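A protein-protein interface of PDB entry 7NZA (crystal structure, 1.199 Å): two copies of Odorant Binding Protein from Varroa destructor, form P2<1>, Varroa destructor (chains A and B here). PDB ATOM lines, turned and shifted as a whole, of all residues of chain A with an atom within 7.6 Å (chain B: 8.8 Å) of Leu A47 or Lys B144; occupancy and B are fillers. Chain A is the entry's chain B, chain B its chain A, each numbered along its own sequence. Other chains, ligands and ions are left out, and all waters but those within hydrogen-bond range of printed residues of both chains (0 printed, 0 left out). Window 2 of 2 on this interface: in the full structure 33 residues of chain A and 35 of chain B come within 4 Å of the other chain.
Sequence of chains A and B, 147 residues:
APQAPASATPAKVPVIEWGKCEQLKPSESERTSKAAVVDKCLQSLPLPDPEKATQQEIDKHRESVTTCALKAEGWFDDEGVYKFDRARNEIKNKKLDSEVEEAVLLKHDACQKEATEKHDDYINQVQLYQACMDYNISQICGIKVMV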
ATOM      1  N   LEU A  42      21.213   2.331 -27.609  1.00  0.00           N
ATOM      2  CA  LEU A  42      20.909   0.990 -28.154  1.00  0.00           C
ATOM      3  C   LEU A  42      21.957   0.482 -29.142  1.00  0.00           C
ATOM      4  O   LEU A  42      22.008  -0.816 -29.222  1.00  0.00           O
ATOM      5  CB  LEU A  42      19.561   1.037 -28.847  1.00  0.00           C
ATOM      6  CG  LEU A  42      18.389   1.077 -27.912  1.00  0.00           C
ATOM      7  CD1 LEU A  42      17.133   1.319 -28.763  1.00  0.00           C
ATOM      8  CD2 LEU A  42      18.265  -0.171 -27.152  1.00  0.00           C
ATOM      9  N   SER A  44      24.965   0.292 -28.666  1.00  0.00           N
ATOM     10  CA  SER A  44      25.886  -0.527 -27.871  1.00  0.00           C
ATOM     11  C   SER A  44      25.202  -1.459 -26.862  1.00  0.00           C
ATOM     12  O   SER A  44      25.912  -2.333 -26.333  1.00  0.00           O
ATOM     13  CB  SER A  44      26.935   0.269 -27.308  1.00  0.00           C
ATOM     14  OG  SER A  44      26.495   1.070 -26.264  1.00  0.00           O
ATOM     15  N   LEU A  45      23.950  -1.230 -26.465  1.00  0.00           N
ATOM     16  CA  LEU A  45      23.216  -1.935 -25.419  1.00  0.00           C
ATOM     17  C   LEU A  45      21.980  -2.564 -26.068  1.00  0.00           C
ATOM     18  O   LEU A  45      20.834  -2.127 -25.907  1.00  0.00           O
ATOM     19  CB  LEU A  45      22.772  -0.954 -24.326  1.00  0.00           C
ATOM     20  CG  LEU A  45      23.913  -0.200 -23.663  1.00  0.00           C
ATOM     21  CD1 LEU A  45      23.397   0.898 -22.735  1.00  0.00           C
ATOM     22  CD2 LEU A  45      24.834  -1.143 -22.900  1.00  0.00           C
ATOM     23  N   PRO A  46      22.178  -3.663 -26.807  1.00  0.00           N
ATOM     24  CA  PRO A  46      21.088  -4.242 -27.549  1.00  0.00           C
ATOM     25  C   PRO A  46      20.033  -4.867 -26.655  1.00  0.00           C
ATOM     26  O   PRO A  46      20.324  -5.389 -25.566  1.00  0.00           O
ATOM     27  CB  PRO A  46      21.803  -5.309 -28.415  1.00  0.00           C
ATOM     28  CG  PRO A  46      23.051  -5.648 -27.681  1.00  0.00           C
ATOM     29  CD  PRO A  46      23.469  -4.357 -27.008  1.00  0.00           C
ATOM     30  N   LEU A  47      18.782  -4.803 -27.063  1.00  0.00           N
ATOM     31  CA  LEU A  47      17.722  -5.490 -26.323  1.00  0.00           C
ATOM     32  C   LEU A  47      17.972  -6.987 -26.264  1.00  0.00           C
ATOM     33  O   LEU A  47      18.316  -7.578 -27.263  1.00  0.00           O
ATOM     34  CB  LEU A  47      16.380  -5.187 -26.985  1.00  0.00           C
ATOM     35  CG  LEU A  47      15.790  -3.814 -26.634  1.00  0.00           C
ATOM     36  CD1 LEU A  47      14.809  -3.419 -27.737  1.00  0.00           C
ATOM     37  CD2 LEU A  47      15.099  -3.740 -25.300  1.00  0.00           C
ATOM     38  N   PRO A  48      17.728  -7.597 -25.085  1.00  0.00           N
ATOM     39  CA  PRO A  48      17.837  -9.054 -25.017  1.00  0.00           C
ATOM     40  C   PRO A  48      16.788  -9.742 -25.899  1.00  0.00           C
ATOM     41  O   PRO A  48      15.747  -9.252 -26.112  1.00  0.00           O
ATOM     42  CB  PRO A  48      17.538  -9.324 -23.543  1.00  0.00           C
ATOM     43  CG  PRO A  48      17.978  -8.047 -22.844  1.00  0.00           C
ATOM     44  CD  PRO A  48      17.491  -6.980 -23.795  1.00  0.00           C
ATOM     45  N   ASP A  49      17.154 -10.888 -26.399  1.00  0.00           N
ATOM     46  CA  ASP A  49      16.292 -11.754 -27.214  1.00  0.00           C
ATOM     47  C   ASP A  49      15.249 -12.332 -26.268  1.00  0.00           C
ATOM     48  O   ASP A  49      15.605 -13.136 -25.432  1.00  0.00           O
ATOM     49  CB  ASP A  49      17.187 -12.879 -27.738  1.00  0.00           C
ATOM     50  CG  ASP A  49      16.491 -13.833 -28.666  1.00  0.00           C
ATOM     51  OD1 ASP A  49      15.253 -13.805 -28.719  1.00  0.00           O
ATOM     52  OD2 ASP A  49      17.248 -14.618 -29.320  1.00  0.00           O
ATOM     53  N   PRO A  50      13.948 -12.056 -26.427  1.00  0.00           N
ATOM     54  CA  PRO A  50      12.981 -12.692 -25.544  1.00  0.00           C
ATOM     55  C   PRO A  50      12.870 -14.226 -25.665  1.00  0.00           C
ATOM     56  O   PRO A  50      12.389 -14.783 -24.738  1.00  0.00           O
ATOM     57  CB  PRO A  50      11.639 -12.081 -25.944  1.00  0.00           C
ATOM     58  CG  PRO A  50      11.876 -11.597 -27.344  1.00  0.00           C
ATOM     59  CD  PRO A  50      13.322 -11.123 -27.362  1.00  0.00           C
ATOM     60  N   ALA A  53      16.066 -14.694 -23.041  1.00  0.00           N
ATOM     61  CA  ALA A  53      16.440 -13.774 -21.938  1.00  0.00           C
ATOM     62  C   ALA A  53      15.762 -14.143 -20.621  1.00  0.00           C
ATOM     63  O   ALA A  53      14.544 -14.295 -20.576  1.00  0.00           O
ATOM     64  CB  ALA A  53      16.053 -12.356 -22.296  1.00  0.00           C
ATOM     65  N   GLU A  57      18.154 -10.500 -16.842  1.00  0.00           N
ATOM     66  CA  GLU A  57      18.831  -9.891 -18.002  1.00  0.00           C
ATOM     67  C   GLU A  57      17.978  -8.758 -18.518  1.00  0.00           C
ATOM     68  O   GLU A  57      18.538  -7.694 -18.869  1.00  0.00           O
ATOM     69  CB  GLU A  57      19.071 -10.922 -19.090  1.00  0.00           C
ATOM     70  CG  GLU A  57      20.224 -11.817 -18.779  1.00  0.00           C
ATOM     71  CD  GLU A  57      20.290 -13.105 -19.554  1.00  0.00           C
ATOM     72  OE1 GLU A  57      19.366 -13.375 -20.302  1.00  0.00           O
ATOM     73  OE2 GLU A  57      21.233 -13.871 -19.261  1.00  0.00           O
ATOM     74  N   ILE A  58      16.687  -8.907 -18.642  1.00  0.00           N
ATOM     75  CA  ILE A  58      15.806  -7.845 -19.164  1.00  0.00           C
ATOM     76  C   ILE A  58      15.879  -6.667 -18.221  1.00  0.00           C
ATOM     77  O   ILE A  58      15.953  -5.474 -18.685  1.00  0.00           O
ATOM     78  CB  ILE A  58      14.382  -8.391 -19.248  1.00  0.00           C
ATOM     79  CG1 ILE A  58      14.347  -9.310 -20.429  1.00  0.00           C
ATOM     80  CG2 ILE A  58      13.358  -7.280 -19.471  1.00  0.00           C
ATOM     81  CD1 ILE A  58      13.146 -10.121 -20.499  1.00  0.00           C
ATOM     82  N   HIS A  61      19.274  -4.871 -18.407  1.00  0.00           N
ATOM     83  CA  HIS A  61      19.336  -4.112 -19.661  1.00  0.00           C
ATOM     84  C   HIS A  61      18.524  -2.833 -19.526  1.00  0.00           C
ATOM     85  O   HIS A  61      19.028  -1.758 -19.944  1.00  0.00           O
ATOM     86  CB  HIS A  61      18.855  -4.928 -20.844  1.00  0.00           C
ATOM     87  CG  HIS A  61      18.735  -4.099 -22.075  1.00  0.00           C
ATOM     88  ND1 HIS A  61      17.589  -3.493 -22.428  1.00  0.00           N
ATOM     89  CD2 HIS A  61      19.688  -3.748 -22.954  1.00  0.00           C
ATOM     90  CE1 HIS A  61      17.848  -2.769 -23.511  1.00  0.00           C
ATOM     91  NE2 HIS A  61      19.114  -2.875 -23.833  1.00  0.00           N
ATOM     92  N   ARG A  62      17.305  -2.893 -19.042  1.00  0.00           N
ATOM     93  CA  ARG A  62      16.545  -1.631 -18.870  1.00  0.00           C
ATOM     94  C   ARG A  62      17.301  -0.632 -17.996  1.00  0.00           C
ATOM     95  O   ARG A  62      17.360   0.579 -18.338  1.00  0.00           O
ATOM     96  CB  ARG A  62      15.211  -2.014 -18.257  1.00  0.00           C
ATOM     97  CG  ARG A  62      14.276  -0.824 -18.133  1.00  0.00           C
ATOM     98  CD  ARG A  62      12.870  -1.307 -17.730  1.00  0.00           C
ATOM     99  NE  ARG A  62      12.973  -1.912 -16.442  1.00  0.00           N
ATOM    100  CZ  ARG A  62      12.830  -3.205 -16.075  1.00  0.00           C
ATOM    101  NH1 ARG A  62      12.499  -4.209 -16.885  1.00  0.00           N
ATOM    102  NH2 ARG A  62      13.011  -3.441 -14.787  1.00  0.00           N
ATOM    103  N   VAL A  65      20.077   1.091 -20.014  1.00  0.00           N
ATOM    104  CA  VAL A  65      19.616   2.141 -20.959  1.00  0.00           C
ATOM    105  C   VAL A  65      19.354   3.425 -20.186  1.00  0.00           C
ATOM    106  O   VAL A  65      19.758   4.493 -20.622  1.00  0.00           O
ATOM    107  CB  VAL A  65      18.408   1.652 -21.761  1.00  0.00           C
ATOM    108  CG1 VAL A  65      17.933   2.803 -22.656  1.00  0.00           C
ATOM    109  CG2 VAL A  65      18.815   0.484 -22.661  1.00  0.00           C
ATOM    110  N   PRO B  14       9.905   5.524 -26.567  1.00  0.00           N
ATOM    111  CA  PRO B  14      10.032   4.125 -26.923  1.00  0.00           C
ATOM    112  C   PRO B  14      11.481   3.711 -27.102  1.00  0.00           C
ATOM    113  O   PRO B  14      12.312   4.464 -27.531  1.00  0.00           O
ATOM    114  CB  PRO B  14       9.268   3.977 -28.244  1.00  0.00           C
ATOM    115  CG  PRO B  14       8.400   5.236 -28.348  1.00  0.00           C
ATOM    116  CD  PRO B  14       9.132   6.292 -27.561  1.00  0.00           C
ATOM    117  N   VAL B  15      11.752   2.478 -26.698  1.00  0.00           N
ATOM    118  CA  VAL B  15      13.081   1.865 -26.790  1.00  0.00           C
ATOM    119  C   VAL B  15      12.946   0.646 -27.693  1.00  0.00           C
ATOM    120  O   VAL B  15      12.434  -0.405 -27.241  1.00  0.00           O
ATOM    121  CB  VAL B  15      13.598   1.504 -25.422  1.00  0.00           C
ATOM    122  CG1 VAL B  15      14.953   0.885 -25.495  1.00  0.00           C
ATOM    123  CG2 VAL B  15      13.647   2.710 -24.489  1.00  0.00           C
ATOM    124  N   ILE B  16      13.266   0.820 -28.956  1.00  0.00           N
ATOM    125  CA  ILE B  16      12.944  -0.123 -30.037  1.00  0.00           C
ATOM    126  C   ILE B  16      14.169  -0.308 -30.898  1.00  0.00           C
ATOM    127  O   ILE B  16      14.777   0.712 -31.291  1.00  0.00           O
ATOM    128  CB  ILE B  16      11.778   0.374 -30.868  1.00  0.00           C
ATOM    129  CG1 ILE B  16      10.579   0.486 -29.959  1.00  0.00           C
ATOM    130  CG2 ILE B  16      11.557  -0.567 -32.017  1.00  0.00           C
ATOM    131  CD1 ILE B  16       9.336   0.989 -30.710  1.00  0.00           C
ATOM    132  N   GLU B  17      14.462  -1.543 -31.235  1.00  0.00           N
ATOM    133  CA  GLU B  17      15.344  -1.895 -32.343  1.00  0.00           C
ATOM    134  C   GLU B  17      14.497  -2.298 -33.535  1.00  0.00           C
ATOM    135  O   GLU B  17      13.646  -3.178 -33.415  1.00  0.00           O
ATOM    136  CB  GLU B  17      16.310  -2.984 -31.953  1.00  0.00           C
ATOM    137  CG  GLU B  17      17.302  -2.512 -30.928  1.00  0.00           C
ATOM    138  CD  GLU B  17      18.453  -3.474 -30.791  1.00  0.00           C
ATOM    139  OE1 GLU B  17      18.534  -4.101 -29.828  1.00  0.00           O
ATOM    140  OE2 GLU B  17      19.371  -3.451 -31.621  1.00  0.00           O
ATOM    141  N   TRP B  18      14.705  -1.672 -34.658  1.00  0.00           N
ATOM    142  CA  TRP B  18      13.831  -1.746 -35.821  1.00  0.00           C
ATOM    143  C   TRP B  18      14.196  -2.893 -36.759  1.00  0.00           C
ATOM    144  O   TRP B  18      13.473  -3.068 -37.728  1.00  0.00           O
ATOM    145  CB  TRP B  18      13.835  -0.385 -36.512  1.00  0.00           C
ATOM    146  CG  TRP B  18      13.125   0.637 -35.667  1.00  0.00           C
ATOM    147  CD1 TRP B  18      13.694   1.497 -34.778  1.00  0.00           C
ATOM    148  CD2 TRP B  18      11.695   0.801 -35.558  1.00  0.00           C
ATOM    149  NE1 TRP B  18      12.705   2.192 -34.128  1.00  0.00           N
ATOM    150  CE2 TRP B  18      11.486   1.783 -34.561  1.00  0.00           C
ATOM    151  CE3 TRP B  18      10.598   0.229 -36.182  1.00  0.00           C
ATOM    152  CZ2 TRP B  18      10.191   2.211 -34.233  1.00  0.00           C
ATOM    153  CZ3 TRP B  18       9.354   0.656 -35.844  1.00  0.00           C
ATOM    154  CH2 TRP B  18       9.153   1.631 -34.871  1.00  0.00           C
ATOM    155  N   GLY B  19      15.288  -3.602 -36.496  1.00  0.00           N
ATOM    156  CA  GLY B  19      15.596  -4.774 -37.320  1.00  0.00           C
ATOM    157  C   GLY B  19      15.798  -4.407 -38.784  1.00  0.00           C
ATOM    158  O   GLY B  19      16.520  -3.489 -39.155  1.00  0.00           O
ATOM    159  N   LYS B  20      15.056  -5.068 -39.632  1.00  0.00           N
ATOM    160  CA  LYS B  20      15.028  -4.949 -41.116  1.00  0.00           C
ATOM    161  C   LYS B  20      14.143  -3.794 -41.561  1.00  0.00           C
ATOM    162  O   LYS B  20      13.906  -3.655 -42.789  1.00  0.00           O
ATOM    163  CB  LYS B  20      14.600  -6.270 -41.789  1.00  0.00           C
ATOM    164  CG  LYS B  20      15.488  -7.455 -41.446  1.00  0.00           C
ATOM    165  CD  LYS B  20      15.156  -8.762 -42.171  1.00  0.00           C
ATOM    166  CE  LYS B  20      13.667  -9.002 -42.316  1.00  0.00           C
ATOM    167  NZ  LYS B  20      13.358 -10.334 -42.893  1.00  0.00           N
ATOM    168  N   ILE B 137       4.195  -7.749 -38.088  1.00  0.00           N
ATOM    169  CA  ILE B 137       5.251  -6.835 -38.568  1.00  0.00           C
ATOM    170  C   ILE B 137       6.483  -7.064 -37.738  1.00  0.00           C
ATOM    171  O   ILE B 137       7.618  -7.107 -38.216  1.00  0.00           O
ATOM    172  CB  ILE B 137       4.809  -5.392 -38.608  1.00  0.00           C
ATOM    173  CG1 ILE B 137       3.713  -5.151 -39.639  1.00  0.00           C
ATOM    174  CG2 ILE B 137       6.031  -4.512 -38.905  1.00  0.00           C
ATOM    175  CD1 ILE B 137       3.161  -3.773 -39.586  1.00  0.00           C
ATOM    176  N   SER B 138       6.329  -7.180 -36.404  1.00  0.00           N
ATOM    177  CA  SER B 138       7.484  -7.382 -35.491  1.00  0.00           C
ATOM    178  C   SER B 138       8.235  -8.652 -35.867  1.00  0.00           C
ATOM    179  O   SER B 138       9.494  -8.686 -35.873  1.00  0.00           O
ATOM    180  CB  SER B 138       7.097  -7.389 -34.025  1.00  0.00           C
ATOM    181  OG  SER B 138       6.584  -6.167 -33.639  1.00  0.00           O
ATOM    182  N   GLN B 139       7.483  -9.712 -36.126  1.00  0.00           N
ATOM    183  CA  GLN B 139       8.103 -10.993 -36.508  1.00  0.00           C
ATOM    184  C   GLN B 139       8.833 -10.887 -37.836  1.00  0.00           C
ATOM    185  O   GLN B 139       9.954 -11.338 -37.933  1.00  0.00           O
ATOM    186  CB  GLN B 139       7.060 -12.116 -36.621  1.00  0.00           C
ATOM    187  CG  GLN B 139       6.385 -12.481 -35.329  1.00  0.00           C
ATOM    188  CD  GLN B 139       7.359 -13.213 -34.444  1.00  0.00           C
ATOM    189  OE1 GLN B 139       7.933 -14.228 -34.831  1.00  0.00           O
ATOM    190  NE2 GLN B 139       7.555 -12.722 -33.246  1.00  0.00           N
ATOM    191  N   CYS B 141      10.024  -8.311 -39.371  1.00  0.00           N
ATOM    192  CA  CYS B 141      11.103  -7.293 -39.385  1.00  0.00           C
ATOM    193  C   CYS B 141      12.209  -7.635 -38.388  1.00  0.00           C
ATOM    194  O   CYS B 141      13.255  -7.014 -38.445  1.00  0.00           O
ATOM    195  CB  CYS B 141      10.498  -5.953 -39.031  1.00  0.00           C
ATOM    196  SG  CYS B 141       9.428  -5.270 -40.313  1.00  0.00           S
ATOM    197  N   GLY B 142      11.934  -8.499 -37.434  1.00  0.00           N
ATOM    198  CA  GLY B 142      12.848  -8.699 -36.280  1.00  0.00           C
ATOM    199  C   GLY B 142      12.902  -7.524 -35.344  1.00  0.00           C
ATOM    200  O   GLY B 142      13.999  -7.169 -34.853  1.00  0.00           O
ATOM    201  N   ILE B 143      11.781  -6.863 -35.125  1.00  0.00           N
ATOM    202  CA  ILE B 143      11.717  -5.706 -34.217  1.00  0.00           C
ATOM    203  C   ILE B 143      11.680  -6.179 -32.784  1.00  0.00           C
ATOM    204  O   ILE B 143      10.979  -7.155 -32.457  1.00  0.00           O
ATOM    205  CB  ILE B 143      10.495  -4.839 -34.499  1.00  0.00           C
ATOM    206  CG1 ILE B 143      10.671  -4.171 -35.858  1.00  0.00           C
ATOM    207  CG2 ILE B 143      10.211  -3.866 -33.390  1.00  0.00           C
ATOM    208  CD1 ILE B 143       9.391  -3.570 -36.420  1.00  0.00           C
ATOM    209  N   LYS B 144      12.463  -5.533 -31.909  1.00  0.00           N
ATOM    210  CA  LYS B 144      12.400  -5.772 -30.453  1.00  0.00           C
ATOM    211  C   LYS B 144      11.962  -4.478 -29.770  1.00  0.00           C
ATOM    212  O   LYS B 144      12.459  -3.433 -30.096  1.00  0.00           O
ATOM    213  CB  LYS B 144      13.743  -6.237 -29.903  1.00  0.00           C
ATOM    214  CG  LYS B 144      14.177  -7.613 -30.377  1.00  0.00           C
ATOM    215  CD  LYS B 144      15.536  -8.024 -29.816  1.00  0.00           C
ATOM    216  CE  LYS B 144      16.665  -7.214 -30.416  1.00  0.00           C
ATOM    217  NZ  LYS B 144      18.027  -7.587 -29.957  1.00  0.00           N
ATOM    218  N   VAL B 145      11.042  -4.607 -28.849  1.00  0.00           N
ATOM    219  CA  VAL B 145      10.522  -3.430 -28.113  1.00  0.00           C
ATOM    220  C   VAL B 145      10.744  -3.690 -26.629  1.00  0.00           C
ATOM    221  O   VAL B 145      10.332  -4.692 -26.141  1.00  0.00           O
ATOM    222  CB  VAL B 145       9.022  -3.208 -28.407  1.00  0.00           C
ATOM    223  CG1 VAL B 145       8.448  -2.012 -27.658  1.00  0.00           C
ATOM    224  CG2 VAL B 145       8.762  -3.093 -29.892  1.00  0.00           C
ATOM    225  N   MET B 146      11.293  -2.706 -25.931  1.00  0.00           N
ATOM    226  CA  MET B 146      11.517  -2.862 -24.479  1.00  0.00           C
ATOM    227  C   MET B 146      10.187  -2.677 -23.755  1.00  0.00           C
ATOM    228  O   MET B 146       9.414  -1.805 -24.152  1.00  0.00           O
ATOM    229  CB  MET B 146      12.488  -1.801 -23.969  1.00  0.00           C
ATOM    230  CG  MET B 146      13.102  -2.150 -22.638  1.00  0.00           C
ATOM    231  SD  MET B 146      14.123  -0.805 -22.014  1.00  0.00           S
ATOM    232  CE  MET B 146      12.804   0.271 -21.496  1.00  0.00           C
ATOM    233  N   VAL B 147       9.852  -3.639 -22.902  1.00  0.00           N
ATOM    234  CA  VAL B 147       8.611  -3.552 -22.106  1.00  0.00           C
ATOM    235  C   VAL B 147       9.170  -3.592 -20.692  1.00  0.00           C
ATOM    236  O   VAL B 147       9.434  -2.519 -20.152  1.00  0.00           O
ATOM    237  CB  VAL B 147       7.637  -4.700 -22.422  1.00  0.00           C
ATOM    238  CG1 VAL B 147       6.963  -4.487 -23.758  1.00  0.00           C
ATOM    239  CG2 VAL B 147       8.320  -6.043 -22.421  1.00  0.00           C
ATOM    240  OXT VAL B 147       9.450  -4.710 -20.225  1.00  0.00           O
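OE1 of Glu B17 sits at hydrogen-bond distance from N of Leu A47. The backbone carbonyl oxygen (O) of Leu A47 sits at hydrogen-bond distance from the side-chain amino group (NZ) of Lys B144, at 2.7 Å.
O of Val B15 is in hydrogen-bond range of N of Met B146, 2.9 Å away. The side-chain carboxylate (OE1) of Glu B17 is in salt-bridge range of the side-chain amino group (NZ) of Lys B144 (3.5 Å). The backbone carbonyl oxygen (O) of Pro A46 sits close to a ring nitrogen (NE2) of His A61 (3.3 Å).
Leu A42 touches Val B15 (CD2 to CG1, 3.9 Å). Leu A42 touches Ile B16. OE1 of Glu B17 touches CA of Pro A46, at 3.4 Å. Leu A47 touches Val B15. Leu A47 touches Met B146 (CD2 to CB, 3.5 Å). Pro A48 touches Lys B144. CE of Met B146 touches CG of Arg A62 (3.8 Å).
Printed residues of chain B within 4 Å of Leu A42: Val B15 (3.9 Å) and Ile B16 (3.5 Å). Leu A45 touches none of the printed residues of chain B. Pro A46 touches just one residue of chain B: Glu B17. Of the printed residues of chain B, Leu A47 touches Val B15, Glu B17, Lys B144 and Met B146. Of the printed residues of chain A, Ile B16 touches Leu A42. Of the printed residues of chain A, Glu B17 touches Pro A46 (3.4 Å) and Leu A47 (2.9 Å). Cys B141 touches none of the printed residues of chain A. Of chain A, only Leu A47 and Pro A48 come within 4 Å of Lys B144. Of the printed residues of chain A, Met B146 touches Leu A47 (3.5 Å) and Arg A62 (3.8 Å). The nearest printed residue of chain B that does not touch Leu A47 is Val B145 (4.1 Å). The nearest printed residue of chain A that does not touch Val B15 is Val A65 (4.5 Å).
Hydrophobic or aromatic side chains of chain B within 4 Å of the printed part of chain A: Val B15 and Met B146. Of the 14 printed residues of chain A, 5 touch a printed residue of chain B. Among the printed residues, 9 pairs touch across the chains.
No position is printed for both chains. Of the 9 pairs that touch across the chains among the printed residues, none has its exchanged pair printed and touching as well.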
